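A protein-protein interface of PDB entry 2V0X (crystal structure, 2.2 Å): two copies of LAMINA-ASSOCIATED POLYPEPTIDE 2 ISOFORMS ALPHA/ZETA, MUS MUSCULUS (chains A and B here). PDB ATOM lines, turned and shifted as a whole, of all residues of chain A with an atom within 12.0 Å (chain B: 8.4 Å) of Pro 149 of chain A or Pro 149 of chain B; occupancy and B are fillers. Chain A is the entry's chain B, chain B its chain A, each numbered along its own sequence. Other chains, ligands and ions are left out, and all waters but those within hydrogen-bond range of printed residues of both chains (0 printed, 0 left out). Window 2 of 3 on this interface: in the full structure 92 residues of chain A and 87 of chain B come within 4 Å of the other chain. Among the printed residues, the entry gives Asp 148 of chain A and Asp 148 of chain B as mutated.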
ATOM      1  N   HIS A   7     -12.114  24.127 -13.914  1.00  0.00           N
ATOM      2  CA  HIS A   7     -10.916  23.291 -13.947  1.00  0.00           C
ATOM      3  C   HIS A   7      -9.949  23.734 -15.046  1.00  0.00           C
ATOM      4  O   HIS A   7      -8.874  23.156 -15.216  1.00  0.00           O
ATOM      5  CB  HIS A   7     -11.291  21.811 -14.126  1.00  0.00           C
ATOM      6  CG  HIS A   7     -11.988  21.505 -15.418  1.00  0.00           C
ATOM      7  ND1 HIS A   7     -11.418  20.729 -16.405  1.00  0.00           N
ATOM      8  CD2 HIS A   7     -13.208  21.866 -15.883  1.00  0.00           C
ATOM      9  CE1 HIS A   7     -12.255  20.626 -17.421  1.00  0.00           C
ATOM     10  NE2 HIS A   7     -13.349  21.307 -17.129  1.00  0.00           N
ATOM     11  N   GLN A 140      -3.704  25.952   1.777  1.00  0.00           N
ATOM     12  CA  GLN A 140      -4.886  26.812   1.873  1.00  0.00           C
ATOM     13  C   GLN A 140      -6.045  26.205   1.087  1.00  0.00           C
ATOM     14  O   GLN A 140      -7.187  26.203   1.550  1.00  0.00           O
ATOM     15  CB  GLN A 140      -4.607  28.225   1.365  1.00  0.00           C
ATOM     16  CG  GLN A 140      -5.655  29.224   1.836  1.00  0.00           C
ATOM     17  CD  GLN A 140      -5.517  30.586   1.194  1.00  0.00           C
ATOM     18  OE1 GLN A 140      -4.418  31.117   1.052  1.00  0.00           O
ATOM     19  NE2 GLN A 140      -6.643  31.162   0.802  1.00  0.00           N
ATOM     20  N   ALA A 141      -5.737  25.680  -0.093  1.00  0.00           N
ATOM     21  CA  ALA A 141      -6.723  25.049  -0.957  1.00  0.00           C
ATOM     22  C   ALA A 141      -7.238  23.771  -0.297  1.00  0.00           C
ATOM     23  O   ALA A 141      -8.429  23.446  -0.377  1.00  0.00           O
ATOM     24  CB  ALA A 141      -6.099  24.722  -2.295  1.00  0.00           C
ATOM     25  N   ALA A 142      -6.320  23.046   0.339  1.00  0.00           N
ATOM     26  CA  ALA A 142      -6.640  21.806   1.036  1.00  0.00           C
ATOM     27  C   ALA A 142      -7.693  22.069   2.107  1.00  0.00           C
ATOM     28  O   ALA A 142      -8.711  21.381   2.160  1.00  0.00           O
ATOM     29  CB  ALA A 142      -5.383  21.210   1.676  1.00  0.00           C
ATOM     30  N   GLN A 143      -7.461  23.090   2.930  1.00  0.00           N
ATOM     31  CA  GLN A 143      -8.387  23.449   4.001  1.00  0.00           C
ATOM     32  C   GLN A 143      -9.775  23.830   3.485  1.00  0.00           C
ATOM     33  O   GLN A 143     -10.788  23.476   4.099  1.00  0.00           O
ATOM     34  CB  GLN A 143      -7.816  24.583   4.849  1.00  0.00           C
ATOM     35  CG  GLN A 143      -6.479  24.247   5.488  1.00  0.00           C
ATOM     36  CD  GLN A 143      -5.985  25.326   6.431  1.00  0.00           C
ATOM     37  OE1 GLN A 143      -6.778  26.040   7.046  1.00  0.00           O
ATOM     38  NE2 GLN A 143      -4.669  25.438   6.562  1.00  0.00           N
ATOM     39  N   ILE A 144      -9.819  24.525   2.350  1.00  0.00           N
ATOM     40  CA  ILE A 144     -11.079  24.946   1.749  1.00  0.00           C
ATOM     41  C   ILE A 144     -11.931  23.741   1.365  1.00  0.00           C
ATOM     42  O   ILE A 144     -13.072  23.617   1.814  1.00  0.00           O
ATOM     43  CB  ILE A 144     -10.831  25.855   0.514  1.00  0.00           C
ATOM     44  CG1 ILE A 144     -10.226  27.180   0.971  1.00  0.00           C
ATOM     45  CG2 ILE A 144     -12.128  26.111  -0.252  1.00  0.00           C
ATOM     46  CD1 ILE A 144      -9.628  28.006  -0.152  1.00  0.00           C
ATOM     47  N   ILE A 145     -11.358  22.828   0.585  1.00  0.00           N
ATOM     48  CA  ILE A 145     -12.077  21.631   0.147  1.00  0.00           C
ATOM     49  C   ILE A 145     -12.263  20.606   1.267  1.00  0.00           C
ATOM     50  O   ILE A 145     -13.030  19.652   1.132  1.00  0.00           O
ATOM     51  CB  ILE A 145     -11.392  20.971  -1.069  1.00  0.00           C
ATOM     52  CG1 ILE A 145      -9.941  20.618  -0.746  1.00  0.00           C
ATOM     53  CG2 ILE A 145     -11.446  21.911  -2.254  1.00  0.00           C
ATOM     54  CD1 ILE A 145      -9.193  19.969  -1.894  1.00  0.00           C
ATOM     55  N   ASN A 146     -11.546  20.821   2.365  1.00  0.00           N
ATOM     56  CA  ASN A 146     -11.608  19.966   3.544  1.00  0.00           C
ATOM     57  C   ASN A 146     -12.775  20.404   4.437  1.00  0.00           C
ATOM     58  O   ASN A 146     -13.417  19.574   5.078  1.00  0.00           O
ATOM     59  CB  ASN A 146     -10.271  20.052   4.292  1.00  0.00           C
ATOM     60  CG  ASN A 146     -10.343  19.539   5.710  1.00  0.00           C
ATOM     61  OD1 ASN A 146      -9.955  18.408   5.993  1.00  0.00           O
ATOM     62  ND2 ASN A 146     -10.764  20.399   6.627  1.00  0.00           N
ATOM     63  N   SER A 147     -13.030  21.711   4.491  1.00  0.00           N
ATOM     64  CA  SER A 147     -14.126  22.249   5.293  1.00  0.00           C
ATOM     65  C   SER A 147     -15.442  22.128   4.518  1.00  0.00           C
ATOM     66  O   SER A 147     -16.043  21.053   4.477  1.00  0.00           O
ATOM     67  CB  SER A 147     -13.855  23.707   5.683  1.00  0.00           C
ATOM     68  OG  SER A 147     -12.663  23.817   6.443  1.00  0.00           O
ATOM     69  N   ASP A 148     -15.889  23.214   3.892  1.00  0.00           N
ATOM     70  CA  ASP A 148     -17.130  23.177   3.126  1.00  0.00           C
ATOM     71  C   ASP A 148     -16.767  23.174   1.639  1.00  0.00           C
ATOM     72  O   ASP A 148     -16.569  24.233   1.036  1.00  0.00           O
ATOM     73  CB  ASP A 148     -18.039  24.325   3.534  1.00  0.00           C
ATOM     74  N   PRO A 149     -16.696  21.975   1.027  1.00  0.00           N
ATOM     75  CA  PRO A 149     -16.358  21.769  -0.386  1.00  0.00           C
ATOM     76  C   PRO A 149     -17.095  22.696  -1.345  1.00  0.00           C
ATOM     77  O   PRO A 149     -16.601  22.991  -2.435  1.00  0.00           O
ATOM     78  CB  PRO A 149     -16.742  20.309  -0.610  1.00  0.00           C
ATOM     79  CG  PRO A 149     -16.436  19.687   0.700  1.00  0.00           C
ATOM     80  CD  PRO A 149     -17.035  20.687   1.660  1.00  0.00           C
ATOM     81  N   SER A 150     -18.268  23.164  -0.931  1.00  0.00           N
ATOM     82  CA  SER A 150     -19.077  24.068  -1.742  1.00  0.00           C
ATOM     83  C   SER A 150     -18.247  25.219  -2.320  1.00  0.00           C
ATOM     84  O   SER A 150     -18.532  25.707  -3.417  1.00  0.00           O
ATOM     85  CB  SER A 150     -20.231  24.628  -0.904  1.00  0.00           C
ATOM     86  OG  SER A 150     -19.748  25.375   0.203  1.00  0.00           O
ATOM     87  N   ASP A 151     -17.201  25.619  -1.597  1.00  0.00           N
ATOM     88  CA  ASP A 151     -16.320  26.707  -2.020  1.00  0.00           C
ATOM     89  C   ASP A 151     -15.373  26.286  -3.148  1.00  0.00           C
ATOM     90  O   ASP A 151     -14.213  26.705  -3.190  1.00  0.00           O
ATOM     91  CB  ASP A 151     -15.528  27.231  -0.826  1.00  0.00           C
ATOM     92  N   ALA A 152     -15.900  25.509  -4.091  1.00  0.00           N
ATOM     93  CA  ALA A 152     -15.142  25.013  -5.231  1.00  0.00           C
ATOM     94  C   ALA A 152     -14.400  26.115  -5.980  1.00  0.00           C
ATOM     95  O   ALA A 152     -13.192  26.014  -6.190  1.00  0.00           O
ATOM     96  CB  ALA A 152     -16.064  24.258  -6.182  1.00  0.00           C
ATOM     97  N   GLN A 153     -15.109  27.172  -6.370  1.00  0.00           N
ATOM     98  CA  GLN A 153     -14.480  28.271  -7.103  1.00  0.00           C
ATOM     99  C   GLN A 153     -13.374  28.953  -6.292  1.00  0.00           C
ATOM    100  O   GLN A 153     -12.420  29.485  -6.856  1.00  0.00           O
ATOM    101  CB  GLN A 153     -15.521  29.299  -7.565  1.00  0.00           C
ATOM    102  CG  GLN A 153     -14.952  30.356  -8.514  1.00  0.00           C
ATOM    103  CD  GLN A 153     -15.992  31.350  -9.000  1.00  0.00           C
ATOM    104  OE1 GLN A 153     -15.988  32.516  -8.606  1.00  0.00           O
ATOM    105  NE2 GLN A 153     -16.884  30.893  -9.869  1.00  0.00           N
ATOM    106  N   GLN A 154     -13.502  28.932  -4.968  1.00  0.00           N
ATOM    107  CA  GLN A 154     -12.496  29.535  -4.101  1.00  0.00           C
ATOM    108  C   GLN A 154     -11.214  28.699  -4.194  1.00  0.00           C
ATOM    109  O   GLN A 154     -10.122  29.238  -4.404  1.00  0.00           O
ATOM    110  CB  GLN A 154     -13.012  29.595  -2.659  1.00  0.00           C
ATOM    111  CG  GLN A 154     -11.981  29.995  -1.608  1.00  0.00           C
ATOM    112  CD  GLN A 154     -11.527  31.440  -1.711  1.00  0.00           C
ATOM    113  OE1 GLN A 154     -11.934  32.285  -0.915  1.00  0.00           O
ATOM    114  NE2 GLN A 154     -10.652  31.724  -2.668  1.00  0.00           N
ATOM    115  N   ALA A 155     -11.357  27.383  -4.072  1.00  0.00           N
ATOM    116  CA  ALA A 155     -10.220  26.475  -4.160  1.00  0.00           C
ATOM    117  C   ALA A 155      -9.612  26.517  -5.568  1.00  0.00           C
ATOM    118  O   ALA A 155      -8.391  26.514  -5.718  1.00  0.00           O
ATOM    119  CB  ALA A 155     -10.643  25.061  -3.799  1.00  0.00           C
ATOM    120  N   LEU A 156     -10.461  26.576  -6.591  1.00  0.00           N
ATOM    121  CA  LEU A 156      -9.999  26.647  -7.973  1.00  0.00           C
ATOM    122  C   LEU A 156      -9.128  27.877  -8.251  1.00  0.00           C
ATOM    123  O   LEU A 156      -8.191  27.808  -9.051  1.00  0.00           O
ATOM    124  CB  LEU A 156     -11.183  26.627  -8.938  1.00  0.00           C
ATOM    125  CG  LEU A 156     -11.747  25.242  -9.250  1.00  0.00           C
ATOM    126  CD1 LEU A 156     -13.194  25.364  -9.710  1.00  0.00           C
ATOM    127  CD2 LEU A 156     -10.883  24.563 -10.311  1.00  0.00           C
ATOM    128  N   ARG A 157      -9.462  29.007  -7.633  1.00  0.00           N
ATOM    129  CA  ARG A 157      -8.674  30.223  -7.809  1.00  0.00           C
ATOM    130  C   ARG A 157      -7.337  30.084  -7.090  1.00  0.00           C
ATOM    131  O   ARG A 157      -6.322  30.586  -7.557  1.00  0.00           O
ATOM    132  CB  ARG A 157      -9.434  31.460  -7.314  1.00  0.00           C
ATOM    133  CG  ARG A 157     -10.318  32.095  -8.397  1.00  0.00           C
ATOM    134  CD  ARG A 157     -11.021  33.372  -7.916  1.00  0.00           C
ATOM    135  NE  ARG A 157     -11.973  33.103  -6.839  1.00  0.00           N
ATOM    136  CZ  ARG A 157     -11.718  33.282  -5.545  1.00  0.00           C
ATOM    137  NH1 ARG A 157     -10.535  33.738  -5.149  1.00  0.00           N
ATOM    138  NH2 ARG A 157     -12.640  32.981  -4.642  1.00  0.00           N
ATOM    139  N   ILE A 158      -7.335  29.379  -5.967  1.00  0.00           N
ATOM    140  CA  ILE A 158      -6.104  29.164  -5.223  1.00  0.00           C
ATOM    141  C   ILE A 158      -5.219  28.239  -6.050  1.00  0.00           C
ATOM    142  O   ILE A 158      -4.049  28.529  -6.269  1.00  0.00           O
ATOM    143  CB  ILE A 158      -6.373  28.559  -3.828  1.00  0.00           C
ATOM    144  CG1 ILE A 158      -7.072  29.595  -2.945  1.00  0.00           C
ATOM    145  CG2 ILE A 158      -5.079  28.163  -3.145  1.00  0.00           C
ATOM    146  CD1 ILE A 158      -6.277  30.879  -2.799  1.00  0.00           C
ATOM    147  N   LEU A 159      -5.826  27.189  -6.595  1.00  0.00           N
ATOM    148  CA  LEU A 159      -5.124  26.210  -7.399  1.00  0.00           C
ATOM    149  C   LEU A 159      -4.656  26.798  -8.716  1.00  0.00           C
ATOM    150  O   LEU A 159      -3.675  26.335  -9.290  1.00  0.00           O
ATOM    151  CB  LEU A 159      -6.001  24.984  -7.668  1.00  0.00           C
ATOM    152  CG  LEU A 159      -6.316  24.027  -6.504  1.00  0.00           C
ATOM    153  CD1 LEU A 159      -7.101  22.844  -7.053  1.00  0.00           C
ATOM    154  CD2 LEU A 159      -5.033  23.537  -5.813  1.00  0.00           C
ATOM    155  N   GLN B 143      -9.533  19.351 -11.620  1.00  0.00           N
ATOM    156  CA  GLN B 143     -10.560  18.602 -12.340  1.00  0.00           C
ATOM    157  C   GLN B 143     -11.457  17.811 -11.403  1.00  0.00           C
ATOM    158  O   GLN B 143     -12.640  17.632 -11.676  1.00  0.00           O
ATOM    159  CB  GLN B 143      -9.921  17.653 -13.358  1.00  0.00           C
ATOM    160  CG  GLN B 143      -9.236  18.356 -14.526  1.00  0.00           C
ATOM    161  CD  GLN B 143      -8.477  17.399 -15.432  1.00  0.00           C
ATOM    162  OE1 GLN B 143      -9.070  16.658 -16.214  1.00  0.00           O
ATOM    163  NE2 GLN B 143      -7.156  17.416 -15.330  1.00  0.00           N
ATOM    164  N   ILE B 144     -10.893  17.327 -10.305  1.00  0.00           N
ATOM    165  CA  ILE B 144     -11.667  16.564  -9.336  1.00  0.00           C
ATOM    166  C   ILE B 144     -12.569  17.510  -8.541  1.00  0.00           C
ATOM    167  O   ILE B 144     -13.776  17.282  -8.427  1.00  0.00           O
ATOM    168  CB  ILE B 144     -10.756  15.794  -8.365  1.00  0.00           C
ATOM    169  CG1 ILE B 144      -9.842  14.836  -9.136  1.00  0.00           C
ATOM    170  CG2 ILE B 144     -11.587  15.066  -7.328  1.00  0.00           C
ATOM    171  CD1 ILE B 144     -10.535  14.076 -10.245  1.00  0.00           C
ATOM    172  N   ILE B 145     -11.979  18.577  -8.007  1.00  0.00           N
ATOM    173  CA  ILE B 145     -12.721  19.562  -7.225  1.00  0.00           C
ATOM    174  C   ILE B 145     -13.892  20.135  -8.022  1.00  0.00           C
ATOM    175  O   ILE B 145     -14.958  20.401  -7.465  1.00  0.00           O
ATOM    176  CB  ILE B 145     -11.788  20.714  -6.761  1.00  0.00           C
ATOM    177  CG1 ILE B 145     -10.890  20.224  -5.622  1.00  0.00           C
ATOM    178  CG2 ILE B 145     -12.592  21.944  -6.334  1.00  0.00           C
ATOM    179  CD1 ILE B 145      -9.830  21.227  -5.199  1.00  0.00           C
ATOM    180  N   ASN B 146     -13.691  20.301  -9.325  1.00  0.00           N
ATOM    181  CA  ASN B 146     -14.719  20.857 -10.199  1.00  0.00           C
ATOM    182  C   ASN B 146     -15.884  19.894 -10.434  1.00  0.00           C
ATOM    183  O   ASN B 146     -17.049  20.303 -10.388  1.00  0.00           O
ATOM    184  CB  ASN B 146     -14.106  21.296 -11.532  1.00  0.00           C
ATOM    185  CG  ASN B 146     -15.008  22.236 -12.310  1.00  0.00           C
ATOM    186  OD1 ASN B 146     -15.418  21.934 -13.429  1.00  0.00           O
ATOM    187  ND2 ASN B 146     -15.296  23.397 -11.733  1.00  0.00           N
ATOM    188  N   SER B 147     -15.576  18.625 -10.689  1.00  0.00           N
ATOM    189  CA  SER B 147     -16.600  17.605 -10.911  1.00  0.00           C
ATOM    190  C   SER B 147     -17.321  17.286  -9.596  1.00  0.00           C
ATOM    191  O   SER B 147     -17.202  16.183  -9.056  1.00  0.00           O
ATOM    192  CB  SER B 147     -15.964  16.336 -11.484  1.00  0.00           C
ATOM    193  OG  SER B 147     -15.354  16.596 -12.739  1.00  0.00           O
ATOM    194  N   ASP B 148     -18.097  18.257  -9.118  1.00  0.00           N
ATOM    195  CA  ASP B 148     -18.859  18.160  -7.874  1.00  0.00           C
ATOM    196  C   ASP B 148     -17.955  18.046  -6.642  1.00  0.00           C
ATOM    197  O   ASP B 148     -17.331  17.007  -6.398  1.00  0.00           O
ATOM    198  CB  ASP B 148     -19.791  16.959  -7.916  1.00  0.00           C
ATOM    199  N   PRO B 149     -17.870  19.133  -5.854  1.00  0.00           N
ATOM    200  CA  PRO B 149     -17.048  19.182  -4.640  1.00  0.00           C
ATOM    201  C   PRO B 149     -17.528  18.196  -3.570  1.00  0.00           C
ATOM    202  O   PRO B 149     -18.189  18.576  -2.599  1.00  0.00           O
ATOM    203  CB  PRO B 149     -17.189  20.640  -4.197  1.00  0.00           C
ATOM    204  CG  PRO B 149     -18.561  21.014  -4.680  1.00  0.00           C
ATOM    205  CD  PRO B 149     -18.570  20.416  -6.061  1.00  0.00           C
ATOM    206  N   SER B 150     -17.202  16.924  -3.774  1.00  0.00           N
ATOM    207  CA  SER B 150     -17.579  15.857  -2.851  1.00  0.00           C
ATOM    208  C   SER B 150     -16.475  14.802  -2.787  1.00  0.00           C
ATOM    209  O   SER B 150     -16.302  14.129  -1.766  1.00  0.00           O
ATOM    210  CB  SER B 150     -18.899  15.215  -3.293  1.00  0.00           C
ATOM    211  OG  SER B 150     -19.920  16.191  -3.438  1.00  0.00           O
ATOM    212  N   ASP B 151     -15.698  14.692  -3.861  1.00  0.00           N
ATOM    213  CA  ASP B 151     -14.599  13.729  -3.934  1.00  0.00           C
ATOM    214  C   ASP B 151     -13.350  14.324  -3.280  1.00  0.00           C
ATOM    215  O   ASP B 151     -12.223  14.088  -3.724  1.00  0.00           O
ATOM    216  CB  ASP B 151     -14.308  13.377  -5.397  1.00  0.00           C
ATOM    217  CG  ASP B 151     -15.577  13.199  -6.215  1.00  0.00           C
ATOM    218  OD1 ASP B 151     -16.417  12.358  -5.836  1.00  0.00           O
ATOM    219  OD2 ASP B 151     -15.741  13.913  -7.228  1.00  0.00           O
ATOM    220  N   ALA B 152     -13.567  15.064  -2.196  1.00  0.00           N
ATOM    221  CA  ALA B 152     -12.501  15.720  -1.457  1.00  0.00           C
ATOM    222  C   ALA B 152     -11.351  14.785  -1.129  1.00  0.00           C
ATOM    223  O   ALA B 152     -10.201  15.100  -1.417  1.00  0.00           O
ATOM    224  CB  ALA B 152     -13.053  16.343  -0.177  1.00  0.00           C
ATOM    225  N   GLN B 153     -11.663  13.618  -0.568  1.00  0.00           N
ATOM    226  CA  GLN B 153     -10.628  12.656  -0.197  1.00  0.00           C
ATOM    227  C   GLN B 153      -9.601  12.384  -1.287  1.00  0.00           C
ATOM    228  O   GLN B 153      -8.403  12.306  -1.015  1.00  0.00           O
ATOM    229  CB  GLN B 153     -11.245  11.342   0.285  1.00  0.00           C
ATOM    230  CG  GLN B 153     -11.700  11.385   1.731  1.00  0.00           C
ATOM    231  CD  GLN B 153     -10.614  11.894   2.667  1.00  0.00           C
ATOM    232  OE1 GLN B 153     -10.879  12.694   3.560  1.00  0.00           O
ATOM    233  NE2 GLN B 153      -9.385  11.441   2.458  1.00  0.00           N
ATOM    234  N   ALA B 155      -8.958  14.374  -4.095  1.00  0.00           N
ATOM    235  CA  ALA B 155      -8.257  15.627  -4.361  1.00  0.00           C
ATOM    236  C   ALA B 155      -7.271  15.967  -3.247  1.00  0.00           C
ATOM    237  O   ALA B 155      -6.177  16.456  -3.514  1.00  0.00           O
ATOM    238  CB  ALA B 155      -9.253  16.765  -4.557  1.00  0.00           C
ATOM    239  N   LEU B 156      -7.639  15.654  -2.010  1.00  0.00           N
ATOM    240  CA  LEU B 156      -6.783  15.925  -0.864  1.00  0.00           C
ATOM    241  C   LEU B 156      -5.563  15.017  -0.854  1.00  0.00           C
ATOM    242  O   LEU B 156      -4.518  15.359  -0.294  1.00  0.00           O
ATOM    243  CB  LEU B 156      -7.551  15.758   0.437  1.00  0.00           C
ATOM    244  CG  LEU B 156      -8.522  16.863   0.829  1.00  0.00           C
ATOM    245  CD1 LEU B 156      -9.073  16.539   2.211  1.00  0.00           C
ATOM    246  CD2 LEU B 156      -7.805  18.204   0.853  1.00  0.00           C
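Of the printed residues of chain B, His 7 of chain A touches Gln 143 (3.7 Å) and Asn 146 (3.3 Å).
Printed residues of chain B within 4 Å of Ala 142 of chain A: Leu 156.
Of the printed residues of chain B, Ile 145 of chain A touches Ile 145, Ala 152 and Leu 156.
No residue of chain B comes within 4 Å of Asp 148 of chain A.
Pro 149 of chain A touches just one residue of chain B: Pro 149.
No residue of chain B comes within 4 Å of Ser 150 of chain A.
Ala 152 of chain A touches none of the printed residues of chain B.
Of chain A, only Ile 145 (3.4 Å) and Leu 159 (3.7 Å) come within 4 Å of Ile 145 of chain B.
No residue of chain A comes within 4 Å of Asp 148 of chain B.
Of the printed residues of chain A, Pro 149 of chain B touches Pro 149 (3.0 Å).
No residue of chain A comes within 4 Å of Ser 150 of chain B.
No residue of chain A comes within 4 Å of Asp 151 of chain B.
Of the printed residues of chain A, Ala 152 of chain B touches Ile 145.
The nearest printed residue of chain A that does not touch Pro 149 of chain B is Ser 150 of chain A (4.3 Å).
The nearest printed residue of chain A that does not touch Asn 146 of chain B is Ala 152 of chain A (5.4 Å).
O of Gln 143 of chain B sits at hydrogen-bond distance from OG of Ser 147 of chain B (3.1 Å).
Of the 13 printed residues of chain B, 6 touch a printed residue of chain A.
Hydrophobic or aromatic side chains of chain B that line the printed part of chain A: Ile 145, Pro 149, Ala 152 and Leu 156.
Printed residues of chain A that touch a printed residue of chain B: His 7, Ala 142, Ile 145, Pro 149, Leu 156 and Leu 159.
Among the printed residues, 9 pairs touch across the chains.
Among the printed residues, no Asp or Glu carboxylate lies within 4 Å of a Lys or Arg side-chain nitrogen of the other chain.
Among the printed residues, pairs that only touch across the chains: His 7 of chain A with Gln 143 of chain B (3.7 Å), His 7 of chain A with Asn 146 of chain B (3.3 Å), Ala 142 of chain A with Leu 156 of chain B (3.6 Å), Ile 145 of chain A with Ile 145 of chain B (3.4 Å), Ile 145 of chain A with Ala 152 of chain B (3.6 Å), Ile 145 of chain A with Leu 156 of chain B (3.5 Å), Pro 149 of chain A with Pro 149 of chain B (3.0 Å), Leu 156 of chain A with Asn 146 of chain B (3.5 Å) and Leu 159 of chain A with Ile 145 of chain B (3.7 Å).
Ile 145 of chain B touches its own counterpart, Ile 145 of chain A.
Ile 145 of chain A touches Leu 156 of chain B, but with the chains exchanged Leu 156 of chain A does not touch Ile 145 of chain B (4.5 Å).
Pro 149 of chain B touches its own counterpart, Pro 149 of chain A.
Leu 156 of chain A touches Asn 146 of chain B, but with the chains exchanged Asn 146 of chain A does not touch Leu 156 of chain B (4.3 Å).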
